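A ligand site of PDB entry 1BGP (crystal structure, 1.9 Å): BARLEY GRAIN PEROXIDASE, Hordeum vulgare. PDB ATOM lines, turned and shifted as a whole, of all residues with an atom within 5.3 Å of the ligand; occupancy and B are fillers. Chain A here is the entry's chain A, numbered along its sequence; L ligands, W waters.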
ATOM      1  N   GLY A  38     -14.905  12.207   3.952  1.00  0.00           N
ATOM      2  CA  GLY A  38     -13.816  11.449   3.355  1.00  0.00           C
ATOM      3  C   GLY A  38     -12.560  12.250   3.075  1.00  0.00           C
ATOM      4  O   GLY A  38     -11.488  11.683   2.874  1.00  0.00           O
ATOM      5  N   ALA A  41      -9.592  11.466   5.420  1.00  0.00           N
ATOM      6  CA  ALA A  41      -8.823  10.287   5.053  1.00  0.00           C
ATOM      7  C   ALA A  41      -7.931  10.607   3.859  1.00  0.00           C
ATOM      8  O   ALA A  41      -6.755  10.233   3.832  1.00  0.00           O
ATOM      9  CB  ALA A  41      -9.760   9.129   4.727  1.00  0.00           C
ATOM     10  N   GLY A  42      -8.485  11.350   2.897  1.00  0.00           N
ATOM     11  CA  GLY A  42      -7.737  11.715   1.706  1.00  0.00           C
ATOM     12  C   GLY A  42      -6.482  12.507   2.021  1.00  0.00           C
ATOM     13  O   GLY A  42      -5.406  12.192   1.518  1.00  0.00           O
ATOM     14  N   LEU A  44      -4.960  12.762   5.015  1.00  0.00           N
ATOM     15  CA  LEU A  44      -4.063  11.962   5.855  1.00  0.00           C
ATOM     16  C   LEU A  44      -3.227  11.017   4.999  1.00  0.00           C
ATOM     17  O   LEU A  44      -2.024  10.904   5.188  1.00  0.00           O
ATOM     18  CB  LEU A  44      -4.879  11.176   6.893  1.00  0.00           C
ATOM     19  CG  LEU A  44      -4.080  10.410   7.942  1.00  0.00           C
ATOM     20  CD1 LEU A  44      -3.163  11.361   8.706  1.00  0.00           C
ATOM     21  CD2 LEU A  44      -5.032   9.706   8.893  1.00  0.00           C
ATOM     22  N   ARG A  45      -3.866  10.367   4.032  1.00  0.00           N
ATOM     23  CA  ARG A  45      -3.150   9.452   3.160  1.00  0.00           C
ATOM     24  C   ARG A  45      -2.192  10.217   2.237  1.00  0.00           C
ATOM     25  O   ARG A  45      -1.095   9.728   1.945  1.00  0.00           O
ATOM     26  CB  ARG A  45      -4.108   8.628   2.320  1.00  0.00           C
ATOM     27  CG  ARG A  45      -3.387   7.603   1.474  1.00  0.00           C
ATOM     28  CD  ARG A  45      -4.116   7.316   0.204  1.00  0.00           C
ATOM     29  NE  ARG A  45      -3.394   6.384  -0.640  1.00  0.00           N
ATOM     30  CZ  ARG A  45      -3.861   5.888  -1.780  1.00  0.00           C
ATOM     31  NH1 ARG A  45      -5.064   6.254  -2.207  1.00  0.00           N
ATOM     32  NH2 ARG A  45      -3.153   5.005  -2.457  1.00  0.00           N
ATOM     33  N   PHE A  48       1.046  10.839   3.942  1.00  0.00           N
ATOM     34  CA  PHE A  48       1.782   9.583   4.023  1.00  0.00           C
ATOM     35  C   PHE A  48       2.427   9.240   2.672  1.00  0.00           C
ATOM     36  O   PHE A  48       3.634   8.990   2.581  1.00  0.00           O
ATOM     37  CB  PHE A  48       0.831   8.451   4.467  1.00  0.00           C
ATOM     38  CG  PHE A  48       1.094   7.112   3.800  1.00  0.00           C
ATOM     39  CD1 PHE A  48       2.249   6.396   4.068  1.00  0.00           C
ATOM     40  CD2 PHE A  48       0.164   6.590   2.908  1.00  0.00           C
ATOM     41  CE1 PHE A  48       2.492   5.168   3.451  1.00  0.00           C
ATOM     42  CE2 PHE A  48       0.396   5.373   2.275  1.00  0.00           C
ATOM     43  CZ  PHE A  48       1.560   4.648   2.550  1.00  0.00           C
ATOM     44  N   PHE A  52       6.606   9.145   1.694  1.00  0.00           N
ATOM     45  CA  PHE A  52       7.349   7.968   1.261  1.00  0.00           C
ATOM     46  C   PHE A  52       7.944   8.086  -0.130  1.00  0.00           C
ATOM     47  O   PHE A  52       9.001   7.523  -0.410  1.00  0.00           O
ATOM     48  CB  PHE A  52       6.505   6.710   1.398  1.00  0.00           C
ATOM     49  CG  PHE A  52       6.522   6.127   2.779  1.00  0.00           C
ATOM     50  CD1 PHE A  52       5.712   6.675   3.774  1.00  0.00           C
ATOM     51  CD2 PHE A  52       7.365   5.070   3.098  1.00  0.00           C
ATOM     52  CE1 PHE A  52       5.757   6.168   5.074  1.00  0.00           C
ATOM     53  CE2 PHE A  52       7.424   4.562   4.394  1.00  0.00           C
ATOM     54  CZ  PHE A  52       6.614   5.110   5.389  1.00  0.00           C
ATOM     55  N   PRO A  76      -6.356   2.013  -9.274  1.00  0.00           N
ATOM     56  CA  PRO A  76      -7.093   2.596  -8.138  1.00  0.00           C
ATOM     57  C   PRO A  76      -6.283   2.757  -6.854  1.00  0.00           C
ATOM     58  O   PRO A  76      -6.370   3.804  -6.200  1.00  0.00           O
ATOM     59  CB  PRO A  76      -8.238   1.613  -7.955  1.00  0.00           C
ATOM     60  CG  PRO A  76      -8.558   1.220  -9.362  1.00  0.00           C
ATOM     61  CD  PRO A  76      -7.170   0.974  -9.931  1.00  0.00           C
ATOM     62  N   ASN A  77      -5.476   1.762  -6.528  1.00  0.00           N
ATOM     63  CA  ASN A  77      -4.663   1.779  -5.316  1.00  0.00           C
ATOM     64  C   ASN A  77      -3.491   2.759  -5.350  1.00  0.00           C
ATOM     65  O   ASN A  77      -2.738   2.879  -4.380  1.00  0.00           O
ATOM     66  CB  ASN A  77      -4.108   0.383  -5.047  1.00  0.00           C
ATOM     67  CG  ASN A  77      -3.254  -0.121  -6.184  1.00  0.00           C
ATOM     68  OD1 ASN A  77      -3.764  -0.602  -7.195  1.00  0.00           O
ATOM     69  ND2 ASN A  77      -1.939   0.015  -6.044  1.00  0.00           N
ATOM     70  N   ARG A  81      -7.108  10.922  -3.850  1.00  0.00           N
ATOM     71  CA  ARG A  81      -8.369  11.651  -3.973  1.00  0.00           C
ATOM     72  C   ARG A  81      -8.187  12.999  -4.648  1.00  0.00           C
ATOM     73  O   ARG A  81      -7.378  13.816  -4.197  1.00  0.00           O
ATOM     74  CB  ARG A  81      -9.013  11.900  -2.614  1.00  0.00           C
ATOM     75  CG  ARG A  81      -9.570  10.674  -1.924  1.00  0.00           C
ATOM     76  CD  ARG A  81     -10.512  11.090  -0.806  1.00  0.00           C
ATOM     77  NE  ARG A  81     -10.869   9.953   0.039  1.00  0.00           N
ATOM     78  CZ  ARG A  81     -12.103   9.605   0.352  1.00  0.00           C
ATOM     79  NH1 ARG A  81     -13.135  10.310  -0.098  1.00  0.00           N
ATOM     80  NH2 ARG A  81     -12.322   8.538   1.117  1.00  0.00           N
ATOM     81  N   PRO A 149       5.395   1.696   0.199  1.00  0.00           N
ATOM     82  CA  PRO A 149       5.006   0.370   0.684  1.00  0.00           C
ATOM     83  C   PRO A 149       3.678  -0.075   0.079  1.00  0.00           C
ATOM     84  O   PRO A 149       2.748   0.724  -0.073  1.00  0.00           O
ATOM     85  CB  PRO A 149       4.890   0.584   2.197  1.00  0.00           C
ATOM     86  CG  PRO A 149       4.498   2.015   2.306  1.00  0.00           C
ATOM     87  CD  PRO A 149       5.394   2.681   1.303  1.00  0.00           C
ATOM     88  N   GLY A 150       3.605  -1.352  -0.311  1.00  0.00           N
ATOM     89  CA  GLY A 150       2.379  -1.884  -0.893  1.00  0.00           C
ATOM     90  C   GLY A 150       1.575  -2.690   0.118  1.00  0.00           C
ATOM     91  O   GLY A 150       2.158  -3.253   1.044  1.00  0.00           O
ATOM     92  N   PRO A 151       0.242  -2.778  -0.051  1.00  0.00           N
ATOM     93  CA  PRO A 151      -0.656  -3.511   0.839  1.00  0.00           C
ATOM     94  C   PRO A 151      -0.438  -5.027   0.923  1.00  0.00           C
ATOM     95  O   PRO A 151      -0.907  -5.666   1.865  1.00  0.00           O
ATOM     96  CB  PRO A 151      -2.038  -3.161   0.282  1.00  0.00           C
ATOM     97  CG  PRO A 151      -1.769  -3.012  -1.173  1.00  0.00           C
ATOM     98  CD  PRO A 151      -0.505  -2.197  -1.170  1.00  0.00           C
ATOM     99  N   LEU A 158       8.170  -4.626   5.342  1.00  0.00           N
ATOM    100  CA  LEU A 158       7.906  -3.265   5.794  1.00  0.00           C
ATOM    101  C   LEU A 158       8.939  -2.752   6.791  1.00  0.00           C
ATOM    102  O   LEU A 158       9.369  -1.600   6.712  1.00  0.00           O
ATOM    103  CB  LEU A 158       6.496  -3.162   6.381  1.00  0.00           C
ATOM    104  CG  LEU A 158       5.344  -3.406   5.399  1.00  0.00           C
ATOM    105  CD1 LEU A 158       4.019  -3.514   6.145  1.00  0.00           C
ATOM    106  CD2 LEU A 158       5.293  -2.287   4.370  1.00  0.00           C
ATOM    107  N   LEU A 162      11.075   0.600   6.140  1.00  0.00           N
ATOM    108  CA  LEU A 162      11.006   1.661   7.136  1.00  0.00           C
ATOM    109  C   LEU A 162      12.320   1.822   7.885  1.00  0.00           C
ATOM    110  O   LEU A 162      12.681   2.927   8.278  1.00  0.00           O
ATOM    111  CB  LEU A 162       9.844   1.431   8.103  1.00  0.00           C
ATOM    112  CG  LEU A 162       8.483   2.016   7.675  1.00  0.00           C
ATOM    113  CD1 LEU A 162       7.977   1.353   6.398  1.00  0.00           C
ATOM    114  CD2 LEU A 162       7.479   1.832   8.793  1.00  0.00           C
ATOM    115  N   LEU A 172       5.963   1.775  12.754  1.00  0.00           N
ATOM    116  CA  LEU A 172       5.174   1.022  11.783  1.00  0.00           C
ATOM    117  C   LEU A 172       3.768   0.730  12.306  1.00  0.00           C
ATOM    118  O   LEU A 172       2.777   1.099  11.665  1.00  0.00           O
ATOM    119  CB  LEU A 172       5.880  -0.286  11.416  1.00  0.00           C
ATOM    120  CG  LEU A 172       5.125  -1.232  10.473  1.00  0.00           C
ATOM    121  CD1 LEU A 172       4.829  -0.540   9.140  1.00  0.00           C
ATOM    122  CD2 LEU A 172       5.922  -2.498  10.232  1.00  0.00           C
ATOM    123  N   ILE A 175       1.851   4.325  12.870  1.00  0.00           N
ATOM    124  CA  ILE A 175       1.385   5.043  11.681  1.00  0.00           C
ATOM    125  C   ILE A 175       0.363   4.243  10.893  1.00  0.00           C
ATOM    126  O   ILE A 175      -0.500   4.814  10.223  1.00  0.00           O
ATOM    127  CB  ILE A 175       2.555   5.529  10.788  1.00  0.00           C
ATOM    128  CG1 ILE A 175       3.325   4.351  10.191  1.00  0.00           C
ATOM    129  CG2 ILE A 175       3.487   6.425  11.593  1.00  0.00           C
ATOM    130  CD1 ILE A 175       4.393   4.781   9.193  1.00  0.00           C
ATOM    131  N   SER A 176       0.425   2.916  10.992  1.00  0.00           N
ATOM    132  CA  SER A 176      -0.537   2.048  10.304  1.00  0.00           C
ATOM    133  C   SER A 176      -1.933   2.302  10.866  1.00  0.00           C
ATOM    134  O   SER A 176      -2.939   1.970  10.241  1.00  0.00           O
ATOM    135  CB  SER A 176      -0.160   0.577  10.466  1.00  0.00           C
ATOM    136  OG  SER A 176       1.024   0.277   9.746  1.00  0.00           O
ATOM    137  N   GLY A 178      -3.382   4.812  10.833  1.00  0.00           N
ATOM    138  CA  GLY A 178      -4.064   5.755   9.953  1.00  0.00           C
ATOM    139  C   GLY A 178      -5.232   5.070   9.262  1.00  0.00           C
ATOM    140  O   GLY A 178      -6.172   5.733   8.834  1.00  0.00           O
ATOM    141  N   HIS A 179      -5.186   3.746   9.199  1.00  0.00           N
ATOM    142  CA  HIS A 179      -6.263   2.965   8.575  1.00  0.00           C
ATOM    143  C   HIS A 179      -7.505   2.861   9.455  1.00  0.00           C
ATOM    144  O   HIS A 179      -8.389   2.048   9.202  1.00  0.00           O
ATOM    145  CB  HIS A 179      -5.762   1.569   8.190  1.00  0.00           C
ATOM    146  CG  HIS A 179      -4.764   1.727   7.060  1.00  0.00           C
ATOM    147  ND1 HIS A 179      -3.965   0.672   6.628  1.00  0.00           N
ATOM    148  CD2 HIS A 179      -4.537   2.839   6.257  1.00  0.00           C
ATOM    149  CE1 HIS A 179      -3.295   1.108   5.551  1.00  0.00           C
ATOM    150  NE2 HIS A 179      -3.620   2.349   5.335  1.00  0.00           N
ATOM    151  N   ILE A 181      -9.512   5.094   9.569  1.00  0.00           N
ATOM    152  CA  ILE A 181     -10.482   5.867   8.798  1.00  0.00           C
ATOM    153  C   ILE A 181     -10.148   5.653   7.319  1.00  0.00           C
ATOM    154  O   ILE A 181      -9.070   5.134   6.997  1.00  0.00           O
ATOM    155  CB  ILE A 181     -10.411   7.391   9.075  1.00  0.00           C
ATOM    156  CG1 ILE A 181      -9.030   7.953   8.741  1.00  0.00           C
ATOM    157  CG2 ILE A 181     -10.816   7.683  10.510  1.00  0.00           C
ATOM    158  CD1 ILE A 181      -8.983   9.461   8.708  1.00  0.00           C
ATOM    159  N   GLY A 182     -11.062   6.009   6.436  1.00  0.00           N
ATOM    160  CA  GLY A 182     -10.788   5.860   5.013  1.00  0.00           C
ATOM    161  C   GLY A 182     -11.357   4.645   4.318  1.00  0.00           C
ATOM    162  O   GLY A 182     -11.963   3.762   4.931  1.00  0.00           O
ATOM    163  N   LEU A 183     -11.093   4.580   3.014  1.00  0.00           N
ATOM    164  CA  LEU A 183     -11.564   3.514   2.144  1.00  0.00           C
ATOM    165  C   LEU A 183     -10.425   2.837   1.387  1.00  0.00           C
ATOM    166  O   LEU A 183      -9.310   3.357   1.298  1.00  0.00           O
ATOM    167  CB  LEU A 183     -12.538   4.099   1.108  1.00  0.00           C
ATOM    168  CG  LEU A 183     -13.722   4.896   1.643  1.00  0.00           C
ATOM    169  CD1 LEU A 183     -14.401   5.628   0.505  1.00  0.00           C
ATOM    170  CD2 LEU A 183     -14.687   3.974   2.359  1.00  0.00           C
ATOM    171  N   ALA A 184     -10.747   1.681   0.810  1.00  0.00           N
ATOM    172  CA  ALA A 184      -9.802   0.917   0.021  1.00  0.00           C
ATOM    173  C   ALA A 184     -10.600   0.243  -1.084  1.00  0.00           C
ATOM    174  O   ALA A 184     -11.724  -0.209  -0.868  1.00  0.00           O
ATOM    175  CB  ALA A 184      -9.115  -0.131   0.875  1.00  0.00           C
ATOM    176  N   HIS A 185     -10.026   0.236  -2.276  1.00  0.00           N
ATOM    177  CA  HIS A 185     -10.632  -0.368  -3.456  1.00  0.00           C
ATOM    178  C   HIS A 185     -10.331  -1.872  -3.445  1.00  0.00           C
ATOM    179  O   HIS A 185      -9.280  -2.297  -2.963  1.00  0.00           O
ATOM    180  CB  HIS A 185     -10.019   0.291  -4.696  1.00  0.00           C
ATOM    181  CG  HIS A 185     -10.693  -0.079  -5.982  1.00  0.00           C
ATOM    182  ND1 HIS A 185     -10.283  -1.130  -6.767  1.00  0.00           N
ATOM    183  CD2 HIS A 185     -11.741   0.483  -6.624  1.00  0.00           C
ATOM    184  CE1 HIS A 185     -11.040  -1.204  -7.845  1.00  0.00           C
ATOM    185  NE2 HIS A 185     -11.932  -0.237  -7.786  1.00  0.00           N
ATOM    186  N   SER A 187      -9.195  -3.839  -5.533  1.00  0.00           N
ATOM    187  CA  SER A 187      -7.896  -4.167  -6.099  1.00  0.00           C
ATOM    188  C   SER A 187      -6.758  -4.262  -5.085  1.00  0.00           C
ATOM    189  O   SER A 187      -5.845  -5.056  -5.252  1.00  0.00           O
ATOM    190  CB  SER A 187      -7.530  -3.170  -7.206  1.00  0.00           C
ATOM    191  OG  SER A 187      -7.672  -1.831  -6.759  1.00  0.00           O
ATOM    192  N   SER A 188      -6.851  -3.486  -4.005  1.00  0.00           N
ATOM    193  CA  SER A 188      -5.817  -3.484  -2.971  1.00  0.00           C
ATOM    194  C   SER A 188      -5.793  -4.722  -2.076  1.00  0.00           C
ATOM    195  O   SER A 188      -4.789  -4.974  -1.402  1.00  0.00           O
ATOM    196  CB  SER A 188      -5.956  -2.238  -2.099  1.00  0.00           C
ATOM    197  OG  SER A 188      -5.715  -1.073  -2.867  1.00  0.00           O
ATOM    198  N   ARG A 221     -15.376  -0.154  -3.488  1.00  0.00           N
ATOM    199  CA  ARG A 221     -14.528   0.183  -2.358  1.00  0.00           C
ATOM    200  C   ARG A 221     -15.224  -0.227  -1.072  1.00  0.00           C
ATOM    201  O   ARG A 221     -16.434  -0.442  -1.052  1.00  0.00           O
ATOM    202  CB  ARG A 221     -14.261   1.678  -2.316  1.00  0.00           C
ATOM    203  CG  ARG A 221     -13.604   2.219  -3.574  1.00  0.00           C
ATOM    204  CD  ARG A 221     -13.563   3.724  -3.573  1.00  0.00           C
ATOM    205  NE  ARG A 221     -13.109   4.235  -4.863  1.00  0.00           N
ATOM    206  CZ  ARG A 221     -11.836   4.306  -5.233  1.00  0.00           C
ATOM    207  NH1 ARG A 221     -10.869   3.907  -4.411  1.00  0.00           N
ATOM    208  NH2 ARG A 221     -11.525   4.768  -6.438  1.00  0.00           N
ATOM    209  N   LEU A 224     -11.678   0.726   5.609  1.00  0.00           N
ATOM    210  CA  LEU A 224     -10.478   0.120   6.152  1.00  0.00           C
ATOM    211  C   LEU A 224     -10.715  -0.373   7.573  1.00  0.00           C
ATOM    212  O   LEU A 224     -10.159  -1.397   7.985  1.00  0.00           O
ATOM    213  CB  LEU A 224      -9.332   1.131   6.119  1.00  0.00           C
ATOM    214  CG  LEU A 224      -8.695   1.377   4.755  1.00  0.00           C
ATOM    215  CD1 LEU A 224      -7.947   2.697   4.756  1.00  0.00           C
ATOM    216  CD2 LEU A 224      -7.757   0.234   4.398  1.00  0.00           C
ATOM    217  N   PHE A 247      -5.733  -5.225   4.676  1.00  0.00           N
ATOM    218  CA  PHE A 247      -4.566  -5.565   3.883  1.00  0.00           C
ATOM    219  C   PHE A 247      -3.679  -6.566   4.595  1.00  0.00           C
ATOM    220  O   PHE A 247      -3.784  -6.754   5.811  1.00  0.00           O
ATOM    221  CB  PHE A 247      -3.703  -4.325   3.613  1.00  0.00           C
ATOM    222  CG  PHE A 247      -4.449  -3.178   2.987  1.00  0.00           C
ATOM    223  CD1 PHE A 247      -5.474  -3.401   2.078  1.00  0.00           C
ATOM    224  CD2 PHE A 247      -4.098  -1.871   3.306  1.00  0.00           C
ATOM    225  CE1 PHE A 247      -6.143  -2.339   1.493  1.00  0.00           C
ATOM    226  CE2 PHE A 247      -4.772  -0.801   2.723  1.00  0.00           C
ATOM    227  CZ  PHE A 247      -5.797  -1.039   1.822  1.00  0.00           C
ATOM    228  N   SER A 249      -0.622  -6.036   4.864  1.00  0.00           N
ATOM    229  CA  SER A 249       0.198  -5.109   5.630  1.00  0.00           C
ATOM    230  C   SER A 249      -0.480  -4.716   6.955  1.00  0.00           C
ATOM    231  O   SER A 249       0.168  -4.243   7.885  1.00  0.00           O
ATOM    232  CB  SER A 249       0.531  -3.863   4.795  1.00  0.00           C
ATOM    233  OG  SER A 249      -0.635  -3.224   4.310  1.00  0.00           O
ATOM    234  N   PHE A 277       1.046   8.196  18.632  1.00  0.00           N
ATOM    235  CA  PHE A 277       0.756   8.624  17.273  1.00  0.00           C
ATOM    236  C   PHE A 277       1.449   9.938  16.903  1.00  0.00           C
ATOM    237  O   PHE A 277       2.091  10.037  15.862  1.00  0.00           O
ATOM    238  CB  PHE A 277      -0.743   8.730  17.008  1.00  0.00           C
ATOM    239  CG  PHE A 277      -1.086   8.987  15.568  1.00  0.00           C
ATOM    240  CD1 PHE A 277      -1.027   7.964  14.632  1.00  0.00           C
ATOM    241  CD2 PHE A 277      -1.448  10.262  15.136  1.00  0.00           C
ATOM    242  CE1 PHE A 277      -1.308   8.197  13.287  1.00  0.00           C
ATOM    243  CE2 PHE A 277      -1.720  10.515  13.791  1.00  0.00           C
ATOM    244  CZ  PHE A 277      -1.657   9.475  12.873  1.00  0.00           C
ATOM    245  N   ILE A 281       4.014   9.755  13.794  1.00  0.00           N
ATOM    246  CA  ILE A 281       3.594  10.463  12.591  1.00  0.00           C
ATOM    247  C   ILE A 281       4.511  11.673  12.418  1.00  0.00           C
ATOM    248  O   ILE A 281       4.751  12.143  11.296  1.00  0.00           O
ATOM    249  CB  ILE A 281       2.103  10.887  12.638  1.00  0.00           C
ATOM    250  CG1 ILE A 281       1.551  11.052  11.222  1.00  0.00           C
ATOM    251  CG2 ILE A 281       1.931  12.184  13.401  1.00  0.00           C
ATOM    252  CD1 ILE A 281       1.449   9.753  10.450  1.00  0.00           C
ATOM    253  N   MET A 284       7.578  10.286  10.725  1.00  0.00           N
ATOM    254  CA  MET A 284       7.255  10.007   9.324  1.00  0.00           C
ATOM    255  C   MET A 284       7.219  11.308   8.524  1.00  0.00           C
ATOM    256  O   MET A 284       7.769  11.395   7.423  1.00  0.00           O
ATOM    257  CB  MET A 284       5.890   9.324   9.209  1.00  0.00           C
ATOM    258  CG  MET A 284       5.469   9.045   7.772  1.00  0.00           C
ATOM    259  SD  MET A 284       3.686   8.799   7.579  1.00  0.00           S
ATOM    260  CE  MET A 284       3.129  10.489   7.517  1.00  0.00           C
HETATM  261  C1  LIG L   1      -5.368   3.969   2.109  1.00  0.00           C
HETATM  262  C2  LIG L   1      -1.447   1.183   1.867  1.00  0.00           C
HETATM  263  C3  LIG L   1       0.347   3.470   5.684  1.00  0.00           C
HETATM  264  C4  LIG L   1      -3.411   6.504   5.694  1.00  0.00           C
HETATM  265  C5  LIG L   1      -4.412   3.084   1.656  1.00  0.00           C
HETATM  266  C6  LIG L   1      -4.558   2.216   0.494  1.00  0.00           C
HETATM  267  C7  LIG L   1      -3.420   1.491   0.368  1.00  0.00           C
HETATM  268  C8  LIG L   1      -2.594   1.872   1.510  1.00  0.00           C
HETATM  269  C9  LIG L   1      -3.120   0.483  -0.715  1.00  0.00           C
HETATM  270  C10 LIG L   1      -5.831   1.938  -0.282  1.00  0.00           C
HETATM  271  C11 LIG L   1      -5.910   2.599  -1.646  1.00  0.00           C
HETATM  272  C12 LIG L   1      -7.164   2.210  -2.400  1.00  0.00           C
HETATM  273  O1  LIG L   1      -7.329   0.999  -2.693  1.00  0.00           O
HETATM  274  O2  LIG L   1      -7.993   3.082  -2.685  1.00  0.00           O
HETATM  275  C13 LIG L   1      -0.713   1.468   3.001  1.00  0.00           C
HETATM  276  C14 LIG L   1       0.479   0.744   3.373  1.00  0.00           C
HETATM  277  C15 LIG L   1       0.986   1.359   4.486  1.00  0.00           C
HETATM  278  C16 LIG L   1       0.076   2.456   4.776  1.00  0.00           C
HETATM  279  C17 LIG L   1       1.012  -0.532   2.754  1.00  0.00           C
HETATM  280  C18 LIG L   1       2.060   0.882   5.247  1.00  0.00           C
HETATM  281  C19 LIG L   1       3.235   1.686   5.535  1.00  0.00           C
HETATM  282  C20 LIG L   1      -0.414   4.608   5.886  1.00  0.00           C
HETATM  283  C21 LIG L   1      -0.078   5.696   6.765  1.00  0.00           C
HETATM  284  C22 LIG L   1      -1.130   6.550   6.790  1.00  0.00           C
HETATM  285  C23 LIG L   1      -2.129   5.970   5.909  1.00  0.00           C
HETATM  286  C24 LIG L   1       1.255   5.903   7.462  1.00  0.00           C
HETATM  287  C25 LIG L   1      -1.221   7.776   7.448  1.00  0.00           C
HETATM  288  C26 LIG L   1      -1.399   7.890   8.881  1.00  0.00           C
HETATM  289  C27 LIG L   1      -4.336   5.924   4.866  1.00  0.00           C
HETATM  290  C28 LIG L   1      -5.682   6.393   4.732  1.00  0.00           C
HETATM  291  C29 LIG L   1      -6.218   5.716   3.692  1.00  0.00           C
HETATM  292  C30 LIG L   1      -5.221   4.793   3.213  1.00  0.00           C
HETATM  293  C31 LIG L   1      -6.430   7.420   5.585  1.00  0.00           C
HETATM  294  C32 LIG L   1      -7.615   5.926   3.129  1.00  0.00           C
HETATM  295  C33 LIG L   1      -7.500   6.973   2.035  1.00  0.00           C
HETATM  296  C34 LIG L   1      -8.843   7.380   1.443  1.00  0.00           C
HETATM  297  O3  LIG L   1      -8.815   8.127   0.447  1.00  0.00           O
HETATM  298  O4  LIG L   1      -9.896   6.962   1.947  1.00  0.00           O
HETATM  299  N1  LIG L   1      -3.205   2.848   2.287  1.00  0.00           N
HETATM  300  N2  LIG L   1      -1.007   2.481   3.895  1.00  0.00           N
HETATM  301  N3  LIG L   1      -1.665   4.800   5.324  1.00  0.00           N
HETATM  302  N4  LIG L   1      -4.079   4.870   4.008  1.00  0.00           N
HETATM  303 FE1  LIG L   1      -2.567   3.639   3.984  1.00  0.00          FE
HETATM  304  O   HOH W   1      -8.542   4.974  -0.767  1.00  0.00           O
HETATM  305  O   HOH W   2      -6.730   8.491  -1.183  1.00  0.00           O
HETATM  306  O   HOH W   3       0.712   2.652  -0.242  1.00  0.00           O
HETATM  307  O   HOH W   4      -7.056   5.255  -4.001  1.00  0.00           O
HETATM  308  O   HOH W   5     -10.250   6.975  -1.623  1.00  0.00           O
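Merely in contact with the ligand: Ala 41 (3.3 Å), Gly 182 (3.4 Å), Gly 150 (3.4 Å), Ile 175 (3.4 Å), Phe 48 (3.5 Å), Pro 149 (3.5 Å), Ser 249 (3.5 Å), Phe 247 (3.6 Å), Gly 178 (3.6 Å), Leu 224 (3.6 Å), Arg 45 (3.6 Å), Ala 184 (3.7 Å), Pro 151 (3.7 Å), Ile 281 (3.7 Å), Ile 181 (3.8 Å), Met 284 (3.8 Å), Leu 44 (3.8 Å), Asn 77 (3.8 Å), Pro 76 (3.9 Å) and Gly 42 (3.95 Å).
Within 4 Å of the ligand: Ala 41, Gly 42, Leu 44, Arg 45, Phe 48, Pro 76, Asn 77, Arg 81, Pro 149, Gly 150, Pro 151, Ile 175, Gly 178, His 179, Ile 181, Gly 182, Leu 183, Ala 184, His 185, Ser 188, Arg 221, Leu 224, Phe 247, Ser 249, Ile 281 and Met 284.
NE of Arg 81 sits close to O of Gly 38, 3.4 Å away.
A ring nitrogen (ND1) of His 185 is in hydrogen-bond range of the side-chain hydroxyl (OG) of Ser 187, at 2.7 Å.
The backbone carbonyl oxygen (O) of Gly 182 sits at hydrogen-bond distance from the backbone NH (N) of Leu 224, 3.1 Å away.
The backbone NH of Ser 249 sits at hydrogen-bond distance from the backbone carbonyl oxygen of Pro 151 (3.0 Å).
The guanidinium group (NH2) of Arg 45 lies within hydrogen-bond range of the backbone carbonyl oxygen (O) of Asn 77 (2.9 Å).
An iron atom (FE1) of the ligand is bound by a ring nitrogen (NE2) of His 179 (2.1 Å).
An oxygen (O1) of the ligand sits at hydrogen-bond distance from the side-chain hydroxyl of Ser 188 (2.6 Å).
An oxygen (O3) of the ligand lies within salt-bridge range of the guanidinium group of Arg 81, at 2.8 Å.
N of His 185 sits at hydrogen-bond distance from O1 of the ligand.
The backbone NH (N) of Leu 183 sits at hydrogen-bond distance from an oxygen (O4) of the ligand (2.9 Å).
O2 of the ligand lies within salt-bridge range of NH1 of Arg 221.
Water W2 lies within hydrogen-bond range of O3 of the ligand and NH1 of Arg 45.
Water W4 lies within hydrogen-bond range of an oxygen (O2) of the ligand (2.7 Å), the backbone carbonyl oxygen of Pro 76 (2.7 Å) and the guanidinium group of Arg 45 (2.9 Å).
Water W1 lies within hydrogen-bond range of O of Leu 183 (2.7 Å) and O2 of the ligand (2.7 Å).
Water W5 bridges O3 of the ligand and NE of Arg 81.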
